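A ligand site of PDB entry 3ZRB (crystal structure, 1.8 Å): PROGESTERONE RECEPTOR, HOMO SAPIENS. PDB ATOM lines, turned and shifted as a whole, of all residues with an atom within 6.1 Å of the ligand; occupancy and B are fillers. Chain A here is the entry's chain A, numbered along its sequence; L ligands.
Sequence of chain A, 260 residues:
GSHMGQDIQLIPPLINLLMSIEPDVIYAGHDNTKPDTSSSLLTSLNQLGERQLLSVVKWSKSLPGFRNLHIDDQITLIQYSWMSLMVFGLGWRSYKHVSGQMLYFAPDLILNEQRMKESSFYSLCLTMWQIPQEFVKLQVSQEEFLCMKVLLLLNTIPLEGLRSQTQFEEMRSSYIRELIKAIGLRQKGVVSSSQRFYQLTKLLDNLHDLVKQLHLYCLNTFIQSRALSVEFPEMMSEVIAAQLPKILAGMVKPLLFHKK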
ATOM      1  N   LEU A  41      14.349  -9.238  26.293  1.00  0.00           N
ATOM      2  CA  LEU A  41      14.271  -9.438  24.845  1.00  0.00           C
ATOM      3  C   LEU A  41      15.598  -9.949  24.313  1.00  0.00           C
ATOM      4  O   LEU A  41      15.668 -10.919  23.573  1.00  0.00           O
ATOM      5  CB  LEU A  41      13.934  -8.135  24.116  1.00  0.00           C
ATOM      6  CG  LEU A  41      13.199  -8.178  22.773  1.00  0.00           C
ATOM      7  CD1 LEU A  41      13.720  -7.067  21.850  1.00  0.00           C
ATOM      8  CD2 LEU A  41      13.186  -9.519  22.062  1.00  0.00           C
ATOM      9  N   LEU A  42      16.672  -9.274  24.696  1.00  0.00           N
ATOM     10  CA  LEU A  42      17.998  -9.683  24.231  1.00  0.00           C
ATOM     11  C   LEU A  42      18.383 -11.068  24.757  1.00  0.00           C
ATOM     12  O   LEU A  42      19.006 -11.833  24.045  1.00  0.00           O
ATOM     13  CB  LEU A  42      19.055  -8.646  24.614  1.00  0.00           C
ATOM     14  CG  LEU A  42      18.776  -7.230  24.102  1.00  0.00           C
ATOM     15  CD1 LEU A  42      19.819  -6.243  24.685  1.00  0.00           C
ATOM     16  CD2 LEU A  42      18.741  -7.216  22.586  1.00  0.00           C
ATOM     17  N   THR A  43      18.050 -11.383  26.000  1.00  0.00           N
ATOM     18  CA  THR A  43      18.312 -12.721  26.525  1.00  0.00           C
ATOM     19  C   THR A  43      17.579 -13.775  25.685  1.00  0.00           C
ATOM     20  O   THR A  43      18.156 -14.804  25.296  1.00  0.00           O
ATOM     21  CB  THR A  43      17.924 -12.770  28.016  1.00  0.00           C
ATOM     22  OG1 THR A  43      18.870 -11.977  28.752  1.00  0.00           O
ATOM     23  CG2 THR A  43      17.911 -14.199  28.568  1.00  0.00           C
ATOM     24  N   LEU A  45      16.508 -13.562  22.515  1.00  0.00           N
ATOM     25  CA  LEU A  45      17.170 -13.656  21.229  1.00  0.00           C
ATOM     26  C   LEU A  45      18.467 -14.479  21.311  1.00  0.00           C
ATOM     27  O   LEU A  45      18.845 -15.183  20.363  1.00  0.00           O
ATOM     28  CB  LEU A  45      17.469 -12.250  20.705  1.00  0.00           C
ATOM     29  CG  LEU A  45      16.229 -11.494  20.203  1.00  0.00           C
ATOM     30  CD1 LEU A  45      16.550 -10.001  19.995  1.00  0.00           C
ATOM     31  CD2 LEU A  45      15.750 -12.140  18.921  1.00  0.00           C
ATOM     32  N   ASN A  46      19.165 -14.387  22.431  1.00  0.00           N
ATOM     33  CA  ASN A  46      20.421 -15.131  22.573  1.00  0.00           C
ATOM     34  C   ASN A  46      20.120 -16.610  22.749  1.00  0.00           C
ATOM     35  O   ASN A  46      20.854 -17.455  22.248  1.00  0.00           O
ATOM     36  CB  ASN A  46      21.219 -14.593  23.754  1.00  0.00           C
ATOM     37  CG  ASN A  46      22.072 -13.398  23.381  1.00  0.00           C
ATOM     38  OD1 ASN A  46      22.222 -13.049  22.202  1.00  0.00           O
ATOM     39  ND2 ASN A  46      22.726 -12.831  24.371  1.00  0.00           N
ATOM     40  N   LEU A  48      17.500 -18.109  21.473  1.00  0.00           N
ATOM     41  CA  LEU A  48      17.161 -18.553  20.114  1.00  0.00           C
ATOM     42  C   LEU A  48      18.443 -18.753  19.288  1.00  0.00           C
ATOM     43  O   LEU A  48      18.597 -19.705  18.507  1.00  0.00           O
ATOM     44  CB  LEU A  48      16.268 -17.530  19.429  1.00  0.00           C
ATOM     45  CG  LEU A  48      15.913 -17.810  17.968  1.00  0.00           C
ATOM     46  CD1 LEU A  48      15.147 -19.124  17.859  1.00  0.00           C
ATOM     47  CD2 LEU A  48      15.125 -16.637  17.356  1.00  0.00           C
ATOM     48  N   GLY A  49      19.387 -17.835  19.486  1.00  0.00           N
ATOM     49  CA  GLY A  49      20.679 -17.929  18.841  1.00  0.00           C
ATOM     50  C   GLY A  49      21.404 -19.210  19.190  1.00  0.00           C
ATOM     51  O   GLY A  49      22.008 -19.845  18.333  1.00  0.00           O
ATOM     52  N   GLN A  52      19.812 -21.965  17.322  1.00  0.00           N
ATOM     53  CA  GLN A  52      20.065 -21.847  15.898  1.00  0.00           C
ATOM     54  C   GLN A  52      21.506 -22.239  15.552  1.00  0.00           C
ATOM     55  O   GLN A  52      21.755 -22.789  14.475  1.00  0.00           O
ATOM     56  CB  GLN A  52      19.769 -20.422  15.415  1.00  0.00           C
ATOM     57  CG  GLN A  52      18.292 -20.112  15.359  1.00  0.00           C
ATOM     58  CD  GLN A  52      18.003 -18.680  14.945  1.00  0.00           C
ATOM     59  OE1 GLN A  52      16.842 -18.270  14.831  1.00  0.00           O
ATOM     60  NE2 GLN A  52      19.057 -17.915  14.714  1.00  0.00           N
ATOM     61  N   TRP A  82      28.648 -17.989  11.305  1.00  0.00           N
ATOM     62  CA  TRP A  82      27.408 -18.254  12.015  1.00  0.00           C
ATOM     63  C   TRP A  82      26.505 -17.036  12.048  1.00  0.00           C
ATOM     64  O   TRP A  82      25.313 -17.184  11.801  1.00  0.00           O
ATOM     65  CB  TRP A  82      27.618 -18.775  13.444  1.00  0.00           C
ATOM     66  CG  TRP A  82      28.277 -17.798  14.300  1.00  0.00           C
ATOM     67  CD1 TRP A  82      29.610 -17.530  14.367  1.00  0.00           C
ATOM     68  CD2 TRP A  82      27.643 -16.911  15.235  1.00  0.00           C
ATOM     69  NE1 TRP A  82      29.847 -16.530  15.262  1.00  0.00           N
ATOM     70  CE2 TRP A  82      28.658 -16.128  15.818  1.00  0.00           C
ATOM     71  CE3 TRP A  82      26.319 -16.713  15.640  1.00  0.00           C
ATOM     72  CZ2 TRP A  82      28.395 -15.167  16.786  1.00  0.00           C
ATOM     73  CZ3 TRP A  82      26.056 -15.745  16.595  1.00  0.00           C
ATOM     74  CH2 TRP A  82      27.094 -14.991  17.161  1.00  0.00           C
ATOM     75  N   MET A  83      27.054 -15.837  12.293  1.00  0.00           N
ATOM     76  CA  MET A  83      26.227 -14.637  12.395  1.00  0.00           C
ATOM     77  C   MET A  83      25.591 -14.361  11.050  1.00  0.00           C
ATOM     78  O   MET A  83      24.406 -14.013  10.992  1.00  0.00           O
ATOM     79  CB  MET A  83      27.048 -13.414  12.816  1.00  0.00           C
ATOM     80  CG  MET A  83      26.296 -12.099  12.729  1.00  0.00           C
ATOM     81  SD  MET A  83      25.256 -11.896  14.176  1.00  0.00           S
ATOM     82  CE  MET A  83      26.552 -11.584  15.387  1.00  0.00           C
ATOM     83  N   MET A  86      22.763 -16.754  10.389  1.00  0.00           N
ATOM     84  CA  MET A  86      21.573 -16.440  11.187  1.00  0.00           C
ATOM     85  C   MET A  86      20.787 -15.263  10.651  1.00  0.00           C
ATOM     86  O   MET A  86      19.566 -15.323  10.567  1.00  0.00           O
ATOM     87  CB  MET A  86      21.905 -16.192  12.672  1.00  0.00           C
ATOM     88  CG  MET A  86      22.112 -17.472  13.425  1.00  0.00           C
ATOM     89  SD  MET A  86      22.492 -17.206  15.153  1.00  0.00           S
ATOM     90  CE  MET A  86      23.460 -18.694  15.478  1.00  0.00           C
ATOM     91  N   VAL A  87      21.478 -14.216  10.223  1.00  0.00           N
ATOM     92  CA  VAL A  87      20.767 -13.026   9.781  1.00  0.00           C
ATOM     93  C   VAL A  87      20.177 -13.286   8.385  1.00  0.00           C
ATOM     94  O   VAL A  87      19.144 -12.758   8.035  1.00  0.00           O
ATOM     95  CB  VAL A  87      21.655 -11.770   9.830  1.00  0.00           C
ATOM     96  CG1 VAL A  87      22.706 -11.775   8.730  1.00  0.00           C
ATOM     97  CG2 VAL A  87      20.799 -10.507   9.766  1.00  0.00           C
ATOM     98  N   LEU A  90      17.086 -15.294   9.164  1.00  0.00           N
ATOM     99  CA  LEU A  90      16.101 -14.304   9.615  1.00  0.00           C
ATOM    100  C   LEU A  90      15.412 -13.595   8.448  1.00  0.00           C
ATOM    101  O   LEU A  90      14.180 -13.449   8.416  1.00  0.00           O
ATOM    102  CB  LEU A  90      16.773 -13.243  10.484  1.00  0.00           C
ATOM    103  CG  LEU A  90      15.963 -12.014  10.861  1.00  0.00           C
ATOM    104  CD1 LEU A  90      14.756 -12.444  11.689  1.00  0.00           C
ATOM    105  CD2 LEU A  90      16.875 -11.079  11.646  1.00  0.00           C
ATOM    106  N   ARG A  93      12.951 -16.002   6.603  1.00  0.00           N
ATOM    107  CA  ARG A  93      11.732 -16.248   7.355  1.00  0.00           C
ATOM    108  C   ARG A  93      10.836 -14.998   7.350  1.00  0.00           C
ATOM    109  O   ARG A  93       9.590 -15.092   7.272  1.00  0.00           O
ATOM    110  CB  ARG A  93      12.067 -16.654   8.806  1.00  0.00           C
ATOM    111  CG  ARG A  93      12.773 -17.998   8.983  1.00  0.00           C
ATOM    112  CD  ARG A  93      12.795 -18.398  10.445  1.00  0.00           C
ATOM    113  NE  ARG A  93      13.606 -17.518  11.298  1.00  0.00           N
ATOM    114  CZ  ARG A  93      14.926 -17.523  11.383  1.00  0.00           C
ATOM    115  NH1 ARG A  93      15.644 -18.371  10.662  1.00  0.00           N
ATOM    116  NH2 ARG A  93      15.529 -16.723  12.262  1.00  0.00           N
ATOM    117  N   PHE A 105      12.022 -13.721  13.849  1.00  0.00           N
ATOM    118  CA  PHE A 105      13.129 -14.442  14.479  1.00  0.00           C
ATOM    119  C   PHE A 105      12.720 -15.895  14.688  1.00  0.00           C
ATOM    120  O   PHE A 105      13.499 -16.815  14.452  1.00  0.00           O
ATOM    121  CB  PHE A 105      13.529 -13.788  15.816  1.00  0.00           C
ATOM    122  CG  PHE A 105      14.219 -12.458  15.652  1.00  0.00           C
ATOM    123  CD1 PHE A 105      15.572 -12.415  15.366  1.00  0.00           C
ATOM    124  CD2 PHE A 105      13.496 -11.280  15.675  1.00  0.00           C
ATOM    125  CE1 PHE A 105      16.197 -11.191  15.185  1.00  0.00           C
ATOM    126  CE2 PHE A 105      14.135 -10.064  15.504  1.00  0.00           C
ATOM    127  CZ  PHE A 105      15.489 -10.035  15.243  1.00  0.00           C
ATOM    128  N   PHE A 121      19.238  -1.063  19.463  1.00  0.00           N
ATOM    129  CA  PHE A 121      18.642  -2.296  18.942  1.00  0.00           C
ATOM    130  C   PHE A 121      17.747  -2.023  17.731  1.00  0.00           C
ATOM    131  O   PHE A 121      17.757  -2.777  16.749  1.00  0.00           O
ATOM    132  CB  PHE A 121      17.842  -3.001  20.043  1.00  0.00           C
ATOM    133  CG  PHE A 121      17.158  -4.237  19.578  1.00  0.00           C
ATOM    134  CD1 PHE A 121      17.893  -5.358  19.239  1.00  0.00           C
ATOM    135  CD2 PHE A 121      15.785  -4.279  19.452  1.00  0.00           C
ATOM    136  CE1 PHE A 121      17.272  -6.499  18.769  1.00  0.00           C
ATOM    137  CE2 PHE A 121      15.150  -5.432  19.008  1.00  0.00           C
ATOM    138  CZ  PHE A 121      15.895  -6.526  18.659  1.00  0.00           C
ATOM    139  N   LEU A 124      19.961  -1.602  14.869  1.00  0.00           N
ATOM    140  CA  LEU A 124      20.450  -2.908  14.465  1.00  0.00           C
ATOM    141  C   LEU A 124      19.384  -3.603  13.616  1.00  0.00           C
ATOM    142  O   LEU A 124      19.679  -4.155  12.569  1.00  0.00           O
ATOM    143  CB  LEU A 124      20.768  -3.755  15.693  1.00  0.00           C
ATOM    144  CG  LEU A 124      21.277  -5.175  15.427  1.00  0.00           C
ATOM    145  CD1 LEU A 124      22.724  -5.084  15.003  1.00  0.00           C
ATOM    146  CD2 LEU A 124      21.119  -6.047  16.653  1.00  0.00           C
ATOM    147  N   MET A 128      19.388  -5.136   9.822  1.00  0.00           N
ATOM    148  CA  MET A 128      19.031  -6.502   9.502  1.00  0.00           C
ATOM    149  C   MET A 128      17.887  -6.540   8.497  1.00  0.00           C
ATOM    150  O   MET A 128      17.835  -7.435   7.664  1.00  0.00           O
ATOM    151  CB  MET A 128      18.642  -7.263  10.772  1.00  0.00           C
ATOM    152  CG  MET A 128      19.821  -7.399  11.703  1.00  0.00           C
ATOM    153  SD  MET A 128      19.535  -8.534  13.070  1.00  0.00           S
ATOM    154  CE  MET A 128      18.193  -7.700  13.880  1.00  0.00           C
ATOM    155  N   LEU A 214      26.673  -6.185  12.808  1.00  0.00           N
ATOM    156  CA  LEU A 214      26.151  -7.164  13.765  1.00  0.00           C
ATOM    157  C   LEU A 214      27.251  -7.705  14.658  1.00  0.00           C
ATOM    158  O   LEU A 214      27.044  -7.900  15.851  1.00  0.00           O
ATOM    159  CB  LEU A 214      25.459  -8.331  13.055  1.00  0.00           C
ATOM    160  CG  LEU A 214      24.400  -8.098  11.972  1.00  0.00           C
ATOM    161  CD1 LEU A 214      23.509  -9.366  11.844  1.00  0.00           C
ATOM    162  CD2 LEU A 214      23.566  -6.832  12.063  1.00  0.00           C
ATOM    163  N   TYR A 217      27.978  -5.062  17.272  1.00  0.00           N
ATOM    164  CA  TYR A 217      26.913  -5.025  18.253  1.00  0.00           C
ATOM    165  C   TYR A 217      27.032  -6.208  19.216  1.00  0.00           C
ATOM    166  O   TYR A 217      26.918  -6.040  20.433  1.00  0.00           O
ATOM    167  CB  TYR A 217      25.577  -5.051  17.543  1.00  0.00           C
ATOM    168  CG  TYR A 217      24.415  -4.902  18.483  1.00  0.00           C
ATOM    169  CD1 TYR A 217      23.911  -6.011  19.147  1.00  0.00           C
ATOM    170  CD2 TYR A 217      23.792  -3.680  18.665  1.00  0.00           C
ATOM    171  CE1 TYR A 217      22.834  -5.909  19.995  1.00  0.00           C
ATOM    172  CE2 TYR A 217      22.703  -3.560  19.507  1.00  0.00           C
ATOM    173  CZ  TYR A 217      22.231  -4.695  20.164  1.00  0.00           C
ATOM    174  OH  TYR A 217      21.142  -4.620  21.004  1.00  0.00           O
ATOM    175  N   CYS A 218      27.308  -7.380  18.666  1.00  0.00           N
ATOM    176  CA  CYS A 218      27.446  -8.604  19.444  1.00  0.00           C
ATOM    177  C   CYS A 218      28.549  -8.497  20.505  1.00  0.00           C
ATOM    178  O   CYS A 218      28.324  -8.715  21.702  1.00  0.00           O
ATOM    179  CB  CYS A 218      27.735  -9.769  18.499  1.00  0.00           C
ATOM    180  SG  CYS A 218      28.027 -11.306  19.373  1.00  0.00           S
ATOM    181  N   LEU A 219      29.745  -8.160  20.055  1.00  0.00           N
ATOM    182  CA  LEU A 219      30.882  -8.054  20.961  1.00  0.00           C
ATOM    183  C   LEU A 219      30.679  -6.985  22.028  1.00  0.00           C
ATOM    184  O   LEU A 219      30.967  -7.218  23.204  1.00  0.00           O
ATOM    185  CB  LEU A 219      32.179  -7.792  20.175  1.00  0.00           C
ATOM    186  CG  LEU A 219      33.462  -8.007  20.962  1.00  0.00           C
ATOM    187  CD1 LEU A 219      33.516  -9.438  21.536  1.00  0.00           C
ATOM    188  CD2 LEU A 219      34.664  -7.714  20.049  1.00  0.00           C
ATOM    189  N   THR A 221      27.779  -6.077  23.212  1.00  0.00           N
ATOM    190  CA  THR A 221      26.764  -6.582  24.130  1.00  0.00           C
ATOM    191  C   THR A 221      27.360  -7.675  25.018  1.00  0.00           C
ATOM    192  O   THR A 221      27.075  -7.749  26.208  1.00  0.00           O
ATOM    193  CB  THR A 221      25.528  -7.100  23.353  1.00  0.00           C
ATOM    194  OG1 THR A 221      25.015  -6.029  22.539  1.00  0.00           O
ATOM    195  CG2 THR A 221      24.449  -7.538  24.319  1.00  0.00           C
ATOM    196  N   PHE A 222      28.243  -8.469  24.437  1.00  0.00           N
ATOM    197  CA  PHE A 222      28.895  -9.587  25.123  1.00  0.00           C
ATOM    198  C   PHE A 222      29.780  -9.061  26.255  1.00  0.00           C
ATOM    199  O   PHE A 222      29.707  -9.549  27.386  1.00  0.00           O
ATOM    200  CB  PHE A 222      29.730 -10.363  24.107  1.00  0.00           C
ATOM    201  CG  PHE A 222      30.368 -11.625  24.640  1.00  0.00           C
ATOM    202  CD1 PHE A 222      29.612 -12.763  24.898  1.00  0.00           C
ATOM    203  CD2 PHE A 222      31.739 -11.696  24.824  1.00  0.00           C
ATOM    204  CE1 PHE A 222      30.202 -13.918  25.378  1.00  0.00           C
ATOM    205  CE2 PHE A 222      32.340 -12.845  25.332  1.00  0.00           C
ATOM    206  CZ  PHE A 222      31.571 -13.965  25.584  1.00  0.00           C
ATOM    207  N   VAL A 230      22.139  -9.280  30.342  1.00  0.00           N
ATOM    208  CA  VAL A 230      21.873 -10.062  29.149  1.00  0.00           C
ATOM    209  C   VAL A 230      22.680 -11.377  29.218  1.00  0.00           C
ATOM    210  O   VAL A 230      23.907 -11.344  29.326  1.00  0.00           O
ATOM    211  CB  VAL A 230      22.280  -9.286  27.886  1.00  0.00           C
ATOM    212  CG1 VAL A 230      22.126 -10.154  26.642  1.00  0.00           C
ATOM    213  CG2 VAL A 230      21.434  -7.998  27.754  1.00  0.00           C
ATOM    214  N   PHE A 232      24.308 -14.811  27.834  1.00  0.00           N
ATOM    215  CA  PHE A 232      24.860 -15.416  26.629  1.00  0.00           C
ATOM    216  C   PHE A 232      25.094 -16.894  26.914  1.00  0.00           C
ATOM    217  O   PHE A 232      25.955 -17.225  27.719  1.00  0.00           O
ATOM    218  CB  PHE A 232      26.191 -14.779  26.263  1.00  0.00           C
ATOM    219  CG  PHE A 232      26.032 -13.510  25.495  1.00  0.00           C
ATOM    220  CD1 PHE A 232      25.746 -12.328  26.157  1.00  0.00           C
ATOM    221  CD2 PHE A 232      26.116 -13.515  24.119  1.00  0.00           C
ATOM    222  CE1 PHE A 232      25.586 -11.164  25.451  1.00  0.00           C
ATOM    223  CE2 PHE A 232      25.940 -12.351  23.398  1.00  0.00           C
ATOM    224  CZ  PHE A 232      25.661 -11.173  24.066  1.00  0.00           C
ATOM    225  N   MET A 236      27.295 -20.278  22.098  1.00  0.00           N
ATOM    226  CA  MET A 236      27.445 -18.980  21.443  1.00  0.00           C
ATOM    227  C   MET A 236      28.614 -18.192  22.049  1.00  0.00           C
ATOM    228  O   MET A 236      29.376 -17.537  21.343  1.00  0.00           O
ATOM    229  CB  MET A 236      26.152 -18.197  21.599  1.00  0.00           C
ATOM    230  CG  MET A 236      26.257 -16.721  21.329  1.00  0.00           C
ATOM    231  SD  MET A 236      24.676 -15.942  21.693  1.00  0.00           S
ATOM    232  CE  MET A 236      23.738 -16.557  20.302  1.00  0.00           C
ATOM    233  N   ILE A 240      31.872 -16.708  19.903  1.00  0.00           N
ATOM    234  CA  ILE A 240      32.212 -15.302  20.074  1.00  0.00           C
ATOM    235  C   ILE A 240      33.643 -15.183  20.607  1.00  0.00           C
ATOM    236  O   ILE A 240      34.469 -14.495  20.006  1.00  0.00           O
ATOM    237  CB  ILE A 240      31.216 -14.613  21.029  1.00  0.00           C
ATOM    238  CG1 ILE A 240      29.812 -14.571  20.408  1.00  0.00           C
ATOM    239  CG2 ILE A 240      31.664 -13.219  21.435  1.00  0.00           C
ATOM    240  CD1 ILE A 240      28.737 -14.176  21.395  1.00  0.00           C
HETATM  241 CL1  LIG L   1      23.051  -9.770  16.543  1.00  0.00          CL
HETATM  242  C1  LIG L   1      21.895  -9.901  17.837  1.00  0.00           C
HETATM  243  N1  LIG L   1      20.559  -9.899  17.662  1.00  0.00           N
HETATM  244  C2  LIG L   1      19.802  -9.786  16.399  1.00  0.00           C
HETATM  245  N2  LIG L   1      19.990 -10.006  18.922  1.00  0.00           N
HETATM  246  C3  LIG L   1      20.932 -10.114  19.819  1.00  0.00           C
HETATM  247  C4  LIG L   1      20.661 -10.244  21.293  1.00  0.00           C
HETATM  248  C5  LIG L   1      22.177 -10.020  19.166  1.00  0.00           C
HETATM  249  S1  LIG L   1      23.787 -10.161  19.897  1.00  0.00           S
HETATM  250  O1  LIG L   1      23.854  -9.314  21.019  1.00  0.00           O
HETATM  251  O2  LIG L   1      24.687 -10.221  18.802  1.00  0.00           O
HETATM  252  N3  LIG L   1      23.745 -11.753  20.376  1.00  0.00           N
HETATM  253  C6  LIG L   1      24.073 -12.854  19.450  1.00  0.00           C
HETATM  254  C7  LIG L   1      23.009 -13.052  18.394  1.00  0.00           C
HETATM  255  C8  LIG L   1      21.658 -13.082  18.760  1.00  0.00           C
HETATM  256  C9  LIG L   1      20.652 -13.265  17.824  1.00  0.00           C
HETATM  257  C10 LIG L   1      23.382 -13.186  17.068  1.00  0.00           C
HETATM  258  C11 LIG L   1      22.393 -13.385  16.114  1.00  0.00           C
HETATM  259  C12 LIG L   1      21.031 -13.389  16.479  1.00  0.00           C
HETATM  260  C13 LIG L   1      20.047 -13.609  15.392  1.00  0.00           C
HETATM  261  C14 LIG L   1      20.062 -13.045  14.143  1.00  0.00           C
HETATM  262  C15 LIG L   1      21.048 -12.024  13.620  1.00  0.00           C
HETATM  263  O3  LIG L   1      19.059 -13.634  13.498  1.00  0.00           O
HETATM  264  N4  LIG L   1      18.457 -14.429  14.195  1.00  0.00           N
HETATM  265  C16 LIG L   1      18.962 -14.530  15.374  1.00  0.00           C
HETATM  266  C17 LIG L   1      18.483 -15.421  16.492  1.00  0.00           C
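O of Met 86 lies close to O3 of the ligand.
Residues that only touch the ligand: Gln 52 (3.1 Å), Met 128 (3.6 Å), Leu 42 (3.6 Å), Leu 45 (3.6 Å), Thr 221 (3.6 Å), Leu 48 (3.7 Å), Met 83 (3.7 Å), Tyr 217 (3.7 Å), Phe 105 (3.7 Å), Trp 82 (3.7 Å), Phe 232 (3.8 Å), Leu 90 (3.8 Å), Met 236 (3.8 Å), Val 87 (3.8 Å), Gly 49 (3.95 Å) and Leu 124 (3.97 Å).
Hydrophobic or aromatic side chains that line the ligand: Leu 42, Leu 45, Leu 48, Trp 82, Met 83, Met 86, Val 87, Leu 90, Phe 105, Leu 124, Met 128, Tyr 217, Phe 232 and Met 236.
19 residues have an atom within 4 Å of the ligand: Leu 42, Leu 45, Asn 46, Leu 48, Gly 49, Gln 52, Trp 82, Met 83, Met 86, Val 87, Leu 90, Phe 105, Leu 124, Met 128, Tyr 217, Cys 218, Thr 221, Phe 232 and Met 236.
An oxygen (O2) of the ligand sits close to the side-chain sulfur of Cys 218, 3.6 Å away.
A nitrogen (N3) of the ligand sits at hydrogen-bond distance from the side-chain amide oxygen (OD1) of Asn 46 (2.7 Å).
The backbone carbonyl oxygen (O) of Phe 105 sits at hydrogen-bond distance from the guanidinium group (NH2) of Arg 93, 3.0 Å away.
The side-chain amide nitrogen (NE2) of Gln 52 lies close to the side-chain sulfur (SD) of Met 86 (3.5 Å).
The guanidinium group (NH2) of Arg 93 sits at hydrogen-bond distance from the side-chain amide oxygen (OE1) of Gln 52 (3.3 Å).
O of Tyr 217 is in hydrogen-bond range of OG1 of Thr 221, 2.8 Å away.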
